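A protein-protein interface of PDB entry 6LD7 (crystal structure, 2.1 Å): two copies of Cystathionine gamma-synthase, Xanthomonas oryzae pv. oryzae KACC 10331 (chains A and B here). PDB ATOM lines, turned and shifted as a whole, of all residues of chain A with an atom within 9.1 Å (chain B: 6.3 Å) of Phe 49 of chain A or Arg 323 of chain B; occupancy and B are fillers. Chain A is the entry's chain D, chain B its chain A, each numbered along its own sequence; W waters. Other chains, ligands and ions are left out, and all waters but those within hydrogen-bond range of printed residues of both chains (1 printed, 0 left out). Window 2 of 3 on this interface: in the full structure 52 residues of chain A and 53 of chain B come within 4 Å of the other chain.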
ATOM      1  N   SER A  45      -3.154  -5.808  -5.185  1.00  0.00           N
ATOM      2  CA  SER A  45      -2.403  -4.787  -5.956  1.00  0.00           C
ATOM      3  C   SER A  45      -3.322  -3.590  -6.196  1.00  0.00           C
ATOM      4  O   SER A  45      -4.541  -3.758  -6.198  1.00  0.00           O
ATOM      5  CB  SER A  45      -1.882  -5.381  -7.242  1.00  0.00           C
ATOM      6  OG  SER A  45      -2.971  -5.633  -8.083  1.00  0.00           O
ATOM      7  N   PHE A  46      -2.764  -2.391  -6.187  1.00  0.00           N
ATOM      8  CA  PHE A  46      -3.366  -1.188  -6.811  1.00  0.00           C
ATOM      9  C   PHE A  46      -3.358  -1.400  -8.334  1.00  0.00           C
ATOM     10  O   PHE A  46      -2.558  -2.163  -8.859  1.00  0.00           O
ATOM     11  CB  PHE A  46      -2.584   0.060  -6.434  1.00  0.00           C
ATOM     12  CG  PHE A  46      -3.034   0.660  -5.127  1.00  0.00           C
ATOM     13  CD1 PHE A  46      -3.206  -0.142  -4.007  1.00  0.00           C
ATOM     14  CD2 PHE A  46      -3.268   2.034  -5.010  1.00  0.00           C
ATOM     15  CE1 PHE A  46      -3.679   0.411  -2.818  1.00  0.00           C
ATOM     16  CE2 PHE A  46      -3.736   2.589  -3.818  1.00  0.00           C
ATOM     17  CZ  PHE A  46      -3.933   1.775  -2.725  1.00  0.00           C
ATOM     18  N   ASP A  47      -4.320  -0.821  -9.042  1.00  0.00           N
ATOM     19  CA  ASP A  47      -4.409  -0.936 -10.524  1.00  0.00           C
ATOM     20  C   ASP A  47      -3.621   0.248 -11.108  1.00  0.00           C
ATOM     21  O   ASP A  47      -4.274   1.210 -11.553  1.00  0.00           O
ATOM     22  CB  ASP A  47      -5.887  -0.956 -10.968  1.00  0.00           C
ATOM     23  CG  ASP A  47      -6.068  -1.184 -12.469  1.00  0.00           C
ATOM     24  OD1 ASP A  47      -5.143  -1.765 -13.098  1.00  0.00           O
ATOM     25  OD2 ASP A  47      -7.130  -0.854 -12.985  1.00  0.00           O
ATOM     26  N   GLY A  48      -2.310   0.273 -10.924  1.00  0.00           N
ATOM     27  CA  GLY A  48      -1.487   1.471 -11.200  1.00  0.00           C
ATOM     28  C   GLY A  48      -1.559   2.516 -10.092  1.00  0.00           C
ATOM     29  O   GLY A  48      -2.426   2.404  -9.156  1.00  0.00           O
ATOM     30  N   PHE A  49      -0.634   3.491 -10.159  1.00  0.00           N
ATOM     31  CA  PHE A  49      -0.453   4.583  -9.183  1.00  0.00           C
ATOM     32  C   PHE A  49      -1.804   5.231  -8.873  1.00  0.00           C
ATOM     33  O   PHE A  49      -2.550   5.574  -9.757  1.00  0.00           O
ATOM     34  CB  PHE A  49       0.585   5.604  -9.665  1.00  0.00           C
ATOM     35  CG  PHE A  49       0.742   6.763  -8.710  1.00  0.00           C
ATOM     36  CD1 PHE A  49      -0.166   7.834  -8.721  1.00  0.00           C
ATOM     37  CD2 PHE A  49       1.748   6.762  -7.754  1.00  0.00           C
ATOM     38  CE1 PHE A  49      -0.060   8.875  -7.806  1.00  0.00           C
ATOM     39  CE2 PHE A  49       1.888   7.833  -6.876  1.00  0.00           C
ATOM     40  CZ  PHE A  49       0.994   8.889  -6.906  1.00  0.00           C
ATOM     41  N   GLY A  50      -2.108   5.357  -7.585  1.00  0.00           N
ATOM     42  CA  GLY A  50      -3.312   6.026  -7.044  1.00  0.00           C
ATOM     43  C   GLY A  50      -4.646   5.367  -7.384  1.00  0.00           C
ATOM     44  O   GLY A  50      -5.618   6.072  -7.197  1.00  0.00           O
ATOM     45  N   ASN A  51      -4.714   4.113  -7.867  1.00  0.00           N
ATOM     46  CA  ASN A  51      -6.001   3.434  -8.211  1.00  0.00           C
ATOM     47  C   ASN A  51      -6.162   2.202  -7.308  1.00  0.00           C
ATOM     48  O   ASN A  51      -5.700   1.123  -7.706  1.00  0.00           O
ATOM     49  CB  ASN A  51      -6.123   2.973  -9.681  1.00  0.00           C
ATOM     50  CG  ASN A  51      -5.775   4.060 -10.666  1.00  0.00           C
ATOM     51  OD1 ASN A  51      -6.288   5.169 -10.551  1.00  0.00           O
ATOM     52  ND2 ASN A  51      -4.874   3.787 -11.599  1.00  0.00           N
ATOM     53  N   LYS A  52      -6.726   2.375  -6.123  1.00  0.00           N
ATOM     54  CA  LYS A  52      -7.150   1.263  -5.268  1.00  0.00           C
ATOM     55  C   LYS A  52      -8.214   0.449  -6.039  1.00  0.00           C
ATOM     56  O   LYS A  52      -9.016   1.031  -6.754  1.00  0.00           O
ATOM     57  CB  LYS A  52      -7.649   1.818  -3.939  1.00  0.00           C
ATOM     58  CG  LYS A  52      -7.578   0.790  -2.812  1.00  0.00           C
ATOM     59  CD  LYS A  52      -8.030   1.348  -1.460  1.00  0.00           C
ATOM     60  CE  LYS A  52      -9.524   1.587  -1.379  1.00  0.00           C
ATOM     61  NZ  LYS A  52     -10.305   0.404  -1.828  1.00  0.00           N
ATOM     62  N   LEU B 315      12.543  10.087  -3.418  1.00  0.00           N
ATOM     63  CA  LEU B 315      12.897  10.236  -4.836  1.00  0.00           C
ATOM     64  C   LEU B 315      12.828  11.711  -5.172  1.00  0.00           C
ATOM     65  O   LEU B 315      11.834  12.342  -4.832  1.00  0.00           O
ATOM     66  CB  LEU B 315      11.885   9.428  -5.633  1.00  0.00           C
ATOM     67  CG  LEU B 315      12.149   9.315  -7.117  1.00  0.00           C
ATOM     68  CD1 LEU B 315      13.442   8.568  -7.372  1.00  0.00           C
ATOM     69  CD2 LEU B 315      11.000   8.583  -7.744  1.00  0.00           C
ATOM     70  N   GLY B 318       9.375  14.845  -7.126  1.00  0.00           N
ATOM     71  CA  GLY B 318       7.984  14.739  -6.641  1.00  0.00           C
ATOM     72  C   GLY B 318       7.177  13.616  -7.298  1.00  0.00           C
ATOM     73  O   GLY B 318       7.737  12.517  -7.701  1.00  0.00           O
ATOM     74  N   GLU B 319       5.876  13.873  -7.354  1.00  0.00           N
ATOM     75  CA  GLU B 319       4.846  12.944  -7.826  1.00  0.00           C
ATOM     76  C   GLU B 319       5.116  12.547  -9.290  1.00  0.00           C
ATOM     77  O   GLU B 319       5.050  11.366  -9.616  1.00  0.00           O
ATOM     78  CB  GLU B 319       3.454  13.522  -7.604  1.00  0.00           C
ATOM     79  CG  GLU B 319       2.483  12.905  -8.589  1.00  0.00           C
ATOM     80  CD  GLU B 319       0.995  13.092  -8.378  1.00  0.00           C
ATOM     81  OE1 GLU B 319       0.568  13.098  -7.203  1.00  0.00           O
ATOM     82  OE2 GLU B 319       0.281  13.154  -9.410  1.00  0.00           O
ATOM     83  N   ALA B 320       5.458  13.421 -10.197  1.00  0.00           N
ATOM     84  CA  ALA B 320       5.713  12.961 -11.574  1.00  0.00           C
ATOM     85  C   ALA B 320       6.858  11.942 -11.578  1.00  0.00           C
ATOM     86  O   ALA B 320       6.815  10.997 -12.383  1.00  0.00           O
ATOM     87  CB  ALA B 320       6.033  14.131 -12.469  1.00  0.00           C
ATOM     88  N   ALA B 321       7.928  12.159 -10.801  1.00  0.00           N
ATOM     89  CA  ALA B 321       9.041  11.167 -10.763  1.00  0.00           C
ATOM     90  C   ALA B 321       8.533   9.816 -10.194  1.00  0.00           C
ATOM     91  O   ALA B 321       8.940   8.796 -10.736  1.00  0.00           O
ATOM     92  CB  ALA B 321      10.201  11.672  -9.966  1.00  0.00           C
ATOM     93  N   VAL B 322       7.664   9.835  -9.170  1.00  0.00           N
ATOM     94  CA  VAL B 322       7.140   8.631  -8.502  1.00  0.00           C
ATOM     95  C   VAL B 322       6.301   7.855  -9.524  1.00  0.00           C
ATOM     96  O   VAL B 322       6.578   6.675  -9.718  1.00  0.00           O
ATOM     97  CB  VAL B 322       6.357   9.023  -7.255  1.00  0.00           C
ATOM     98  CG1 VAL B 322       5.517   7.881  -6.715  1.00  0.00           C
ATOM     99  CG2 VAL B 322       7.275   9.597  -6.213  1.00  0.00           C
ATOM    100  N   ARG B 323       5.424   8.514 -10.271  1.00  0.00           N
ATOM    101  CA  ARG B 323       4.585   7.833 -11.285  1.00  0.00           C
ATOM    102  C   ARG B 323       5.496   7.176 -12.327  1.00  0.00           C
ATOM    103  O   ARG B 323       5.270   6.000 -12.678  1.00  0.00           O
ATOM    104  CB  ARG B 323       3.631   8.772 -12.008  1.00  0.00           C
ATOM    105  CG  ARG B 323       2.535   9.330 -11.124  1.00  0.00           C
ATOM    106  CD  ARG B 323       1.809  10.381 -11.977  1.00  0.00           C
ATOM    107  NE  ARG B 323       0.670  10.834 -11.202  1.00  0.00           N
ATOM    108  CZ  ARG B 323      -0.499  10.201 -11.168  1.00  0.00           C
ATOM    109  NH1 ARG B 323      -0.706   9.119 -11.902  1.00  0.00           N
ATOM    110  NH2 ARG B 323      -1.467  10.662 -10.403  1.00  0.00           N
ATOM    111  N   ALA B 324       6.523   7.867 -12.801  1.00  0.00           N
ATOM    112  CA  ALA B 324       7.398   7.239 -13.817  1.00  0.00           C
ATOM    113  C   ALA B 324       8.182   6.072 -13.161  1.00  0.00           C
ATOM    114  O   ALA B 324       8.384   5.006 -13.786  1.00  0.00           O
ATOM    115  CB  ALA B 324       8.294   8.299 -14.413  1.00  0.00           C
ATOM    116  N   PHE B 325       8.697   6.256 -11.938  1.00  0.00           N
ATOM    117  CA  PHE B 325       9.390   5.163 -11.200  1.00  0.00           C
ATOM    118  C   PHE B 325       8.492   3.918 -11.151  1.00  0.00           C
ATOM    119  O   PHE B 325       8.977   2.802 -11.517  1.00  0.00           O
ATOM    120  CB  PHE B 325       9.767   5.658  -9.800  1.00  0.00           C
ATOM    121  CG  PHE B 325      10.622   4.692  -9.049  1.00  0.00           C
ATOM    122  CD1 PHE B 325      10.060   3.605  -8.404  1.00  0.00           C
ATOM    123  CD2 PHE B 325      12.000   4.860  -9.024  1.00  0.00           C
ATOM    124  CE1 PHE B 325      10.884   2.694  -7.773  1.00  0.00           C
ATOM    125  CE2 PHE B 325      12.814   3.968  -8.349  1.00  0.00           C
ATOM    126  CZ  PHE B 325      12.242   2.912  -7.692  1.00  0.00           C
ATOM    127  N   VAL B 326       7.262   4.018 -10.643  1.00  0.00           N
ATOM    128  CA  VAL B 326       6.434   2.787 -10.394  1.00  0.00           C
ATOM    129  C   VAL B 326       5.882   2.195 -11.694  1.00  0.00           C
ATOM    130  O   VAL B 326       5.804   0.948 -11.767  1.00  0.00           O
ATOM    131  CB  VAL B 326       5.325   2.979  -9.365  1.00  0.00           C
ATOM    132  CG1 VAL B 326       5.850   3.744  -8.163  1.00  0.00           C
ATOM    133  CG2 VAL B 326       4.146   3.654  -9.960  1.00  0.00           C
ATOM    134  N   ASP B 327       5.780   2.985 -12.759  1.00  0.00           N
ATOM    135  CA  ASP B 327       5.161   2.549 -14.045  1.00  0.00           C
ATOM    136  C   ASP B 327       5.793   1.231 -14.506  1.00  0.00           C
ATOM    137  O   ASP B 327       5.162   0.156 -14.261  1.00  0.00           O
ATOM    138  CB  ASP B 327       5.083   3.678 -15.081  1.00  0.00           C
ATOM    139  CG  ASP B 327       4.266   3.340 -16.343  1.00  0.00           C
ATOM    140  OD1 ASP B 327       3.869   2.195 -16.541  1.00  0.00           O
ATOM    141  OD2 ASP B 327       4.087   4.222 -17.150  1.00  0.00           O
ATOM    142  N   GLY B 328       6.959   1.121 -15.083  1.00  0.00           N
ATOM    143  CA  GLY B 328       7.238  -0.315 -15.463  1.00  0.00           C
ATOM    144  C   GLY B 328       7.870  -1.287 -14.434  1.00  0.00           C
ATOM    145  O   GLY B 328       8.671  -2.123 -14.875  1.00  0.00           O
ATOM    146  N   LEU B 334       2.933  -2.991  -6.516  1.00  0.00           N
ATOM    147  CA  LEU B 334       2.361  -1.811  -5.817  1.00  0.00           C
ATOM    148  C   LEU B 334       1.198  -2.246  -4.945  1.00  0.00           C
ATOM    149  O   LEU B 334       0.083  -2.551  -5.496  1.00  0.00           O
ATOM    150  CB  LEU B 334       1.898  -0.805  -6.876  1.00  0.00           C
ATOM    151  CG  LEU B 334       1.420   0.525  -6.328  1.00  0.00           C
ATOM    152  CD1 LEU B 334       2.543   1.275  -5.662  1.00  0.00           C
ATOM    153  CD2 LEU B 334       0.817   1.313  -7.513  1.00  0.00           C
ATOM    154  N   HIS B 347       3.529   3.911  -1.782  1.00  0.00           N
ATOM    155  CA  HIS B 347       3.762   5.376  -1.796  1.00  0.00           C
ATOM    156  C   HIS B 347       2.923   5.913  -0.662  1.00  0.00           C
ATOM    157  O   HIS B 347       1.711   6.008  -0.847  1.00  0.00           O
ATOM    158  CB  HIS B 347       3.335   5.937  -3.163  1.00  0.00           C
ATOM    159  CG  HIS B 347       3.424   7.421  -3.270  1.00  0.00           C
ATOM    160  ND1 HIS B 347       2.287   8.224  -3.425  1.00  0.00           N
ATOM    161  CD2 HIS B 347       4.499   8.243  -3.290  1.00  0.00           C
ATOM    162  CE1 HIS B 347       2.691   9.490  -3.484  1.00  0.00           C
ATOM    163  NE2 HIS B 347       4.047   9.533  -3.423  1.00  0.00           N
ATOM    164  N   SER B 350      -0.154   8.631  -1.256  1.00  0.00           N
ATOM    165  CA  SER B 350      -1.391   8.130  -1.910  1.00  0.00           C
ATOM    166  C   SER B 350      -1.910   6.790  -1.345  1.00  0.00           C
ATOM    167  O   SER B 350      -2.854   6.224  -1.940  1.00  0.00           O
ATOM    168  CB  SER B 350      -1.142   7.977  -3.367  1.00  0.00           C
ATOM    169  OG  SER B 350      -0.231   6.922  -3.637  1.00  0.00           O
ATOM    170  N   ARG B 393      13.752   6.064 -15.323  1.00  0.00           N
ATOM    171  CA  ARG B 393      12.453   6.613 -15.718  1.00  0.00           C
ATOM    172  C   ARG B 393      12.165   7.874 -14.894  1.00  0.00           C
ATOM    173  O   ARG B 393      11.691   8.874 -15.491  1.00  0.00           O
ATOM    174  CB  ARG B 393      11.323   5.594 -15.615  1.00  0.00           C
ATOM    175  CG  ARG B 393      11.433   4.385 -16.546  1.00  0.00           C
ATOM    176  CD  ARG B 393      10.177   3.542 -16.422  1.00  0.00           C
ATOM    177  NE  ARG B 393       9.955   2.973 -15.070  1.00  0.00           N
ATOM    178  CZ  ARG B 393      10.382   1.760 -14.679  1.00  0.00           C
ATOM    179  NH1 ARG B 393      11.154   1.052 -15.486  1.00  0.00           N
ATOM    180  NH2 ARG B 393      10.100   1.272 -13.463  1.00  0.00           N
HETATM  181  O   HOH W   1      -0.511   4.543  -5.287  1.00  0.00           O
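Ser 45 of chain A touches Leu 334 of chain B (CA to O, 3.4 Å). Gly 48 of chain A touches Leu 334 of chain B (C to CD2, 3.7 Å). Val 322 of chain B touches Phe 49 of chain A (CG1 to CE2, 3.6 Å). Phe 49 of chain A touches Arg 323 of chain B. Leu 334 of chain B touches Phe 49 of chain A. His 347 of chain B touches Phe 49 of chain A. OG of Ser 350 of chain B touches CE2 of Phe 49 of chain A (3.98 Å).
Of chain B, only Val 322, Arg 323, Leu 334, His 347 and Ser 350 come within 4 Å of Phe 49 of chain A. Printed residues of chain A within 4 Å of Arg 323 of chain B: Phe 49 (3.4 Å). Of chain A, only Phe 49 comes within 4 Å of Val 322 of chain B. No residue of chain A comes within 4 Å of Ala 324 of chain B. Of the printed residues of chain A, Leu 334 of chain B touches Ser 45 (3.4 Å), Phe 46 (2.9 Å), Gly 48 (3.7 Å) and Phe 49 (3.7 Å). Printed residues of chain B within 4 Å of Gly 48 of chain A: Leu 334 (3.7 Å). Printed residues of chain B within 4 Å of Phe 46 of chain A: Leu 334 (2.9 Å). The nearest residue of chain B that does not touch Phe 49 of chain A is Val 326 of chain B (4.1 Å). The nearest residue of chain A that does not touch Arg 323 of chain B is Gly 50 of chain A (5.9 Å).
The backbone carbonyl oxygen (O) of Leu 334 of chain B sits at hydrogen-bond distance from the backbone NH (N) of Phe 46 of chain A (2.9 Å).
Water W1 bridges OG of Ser 350 of chain B (2.9 Å) and N of Gly 50 of chain A (2.9 Å).
No position is printed for both chains. Of the 8 pairs that touch across the chains among the printed residues, none has its exchanged pair printed and touching as well.
OE2 of Glu 319 of chain B lies within salt-bridge range of NE of Arg 323 of chain B, at 3.0 Å. ND1 of His 347 of chain B is in hydrogen-bond range of OG of Ser 350 of chain B (2.8 Å). The backbone carbonyl oxygen (O) of Phe 49 of chain A is in hydrogen-bond range of the side-chain amide nitrogen (ND2) of Asn 51 of chain A, 3.5 Å away.
Of the 16 printed residues of chain B, 5 touch a printed residue of chain A. Hydrophobic or aromatic side chains of chain B within 4 Å of the printed part of chain A: Val 322, Leu 334 and His 347. Among the printed residues, no Asp or Glu carboxylate lies within 4 Å of a Lys or Arg side-chain nitrogen of the other chain.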
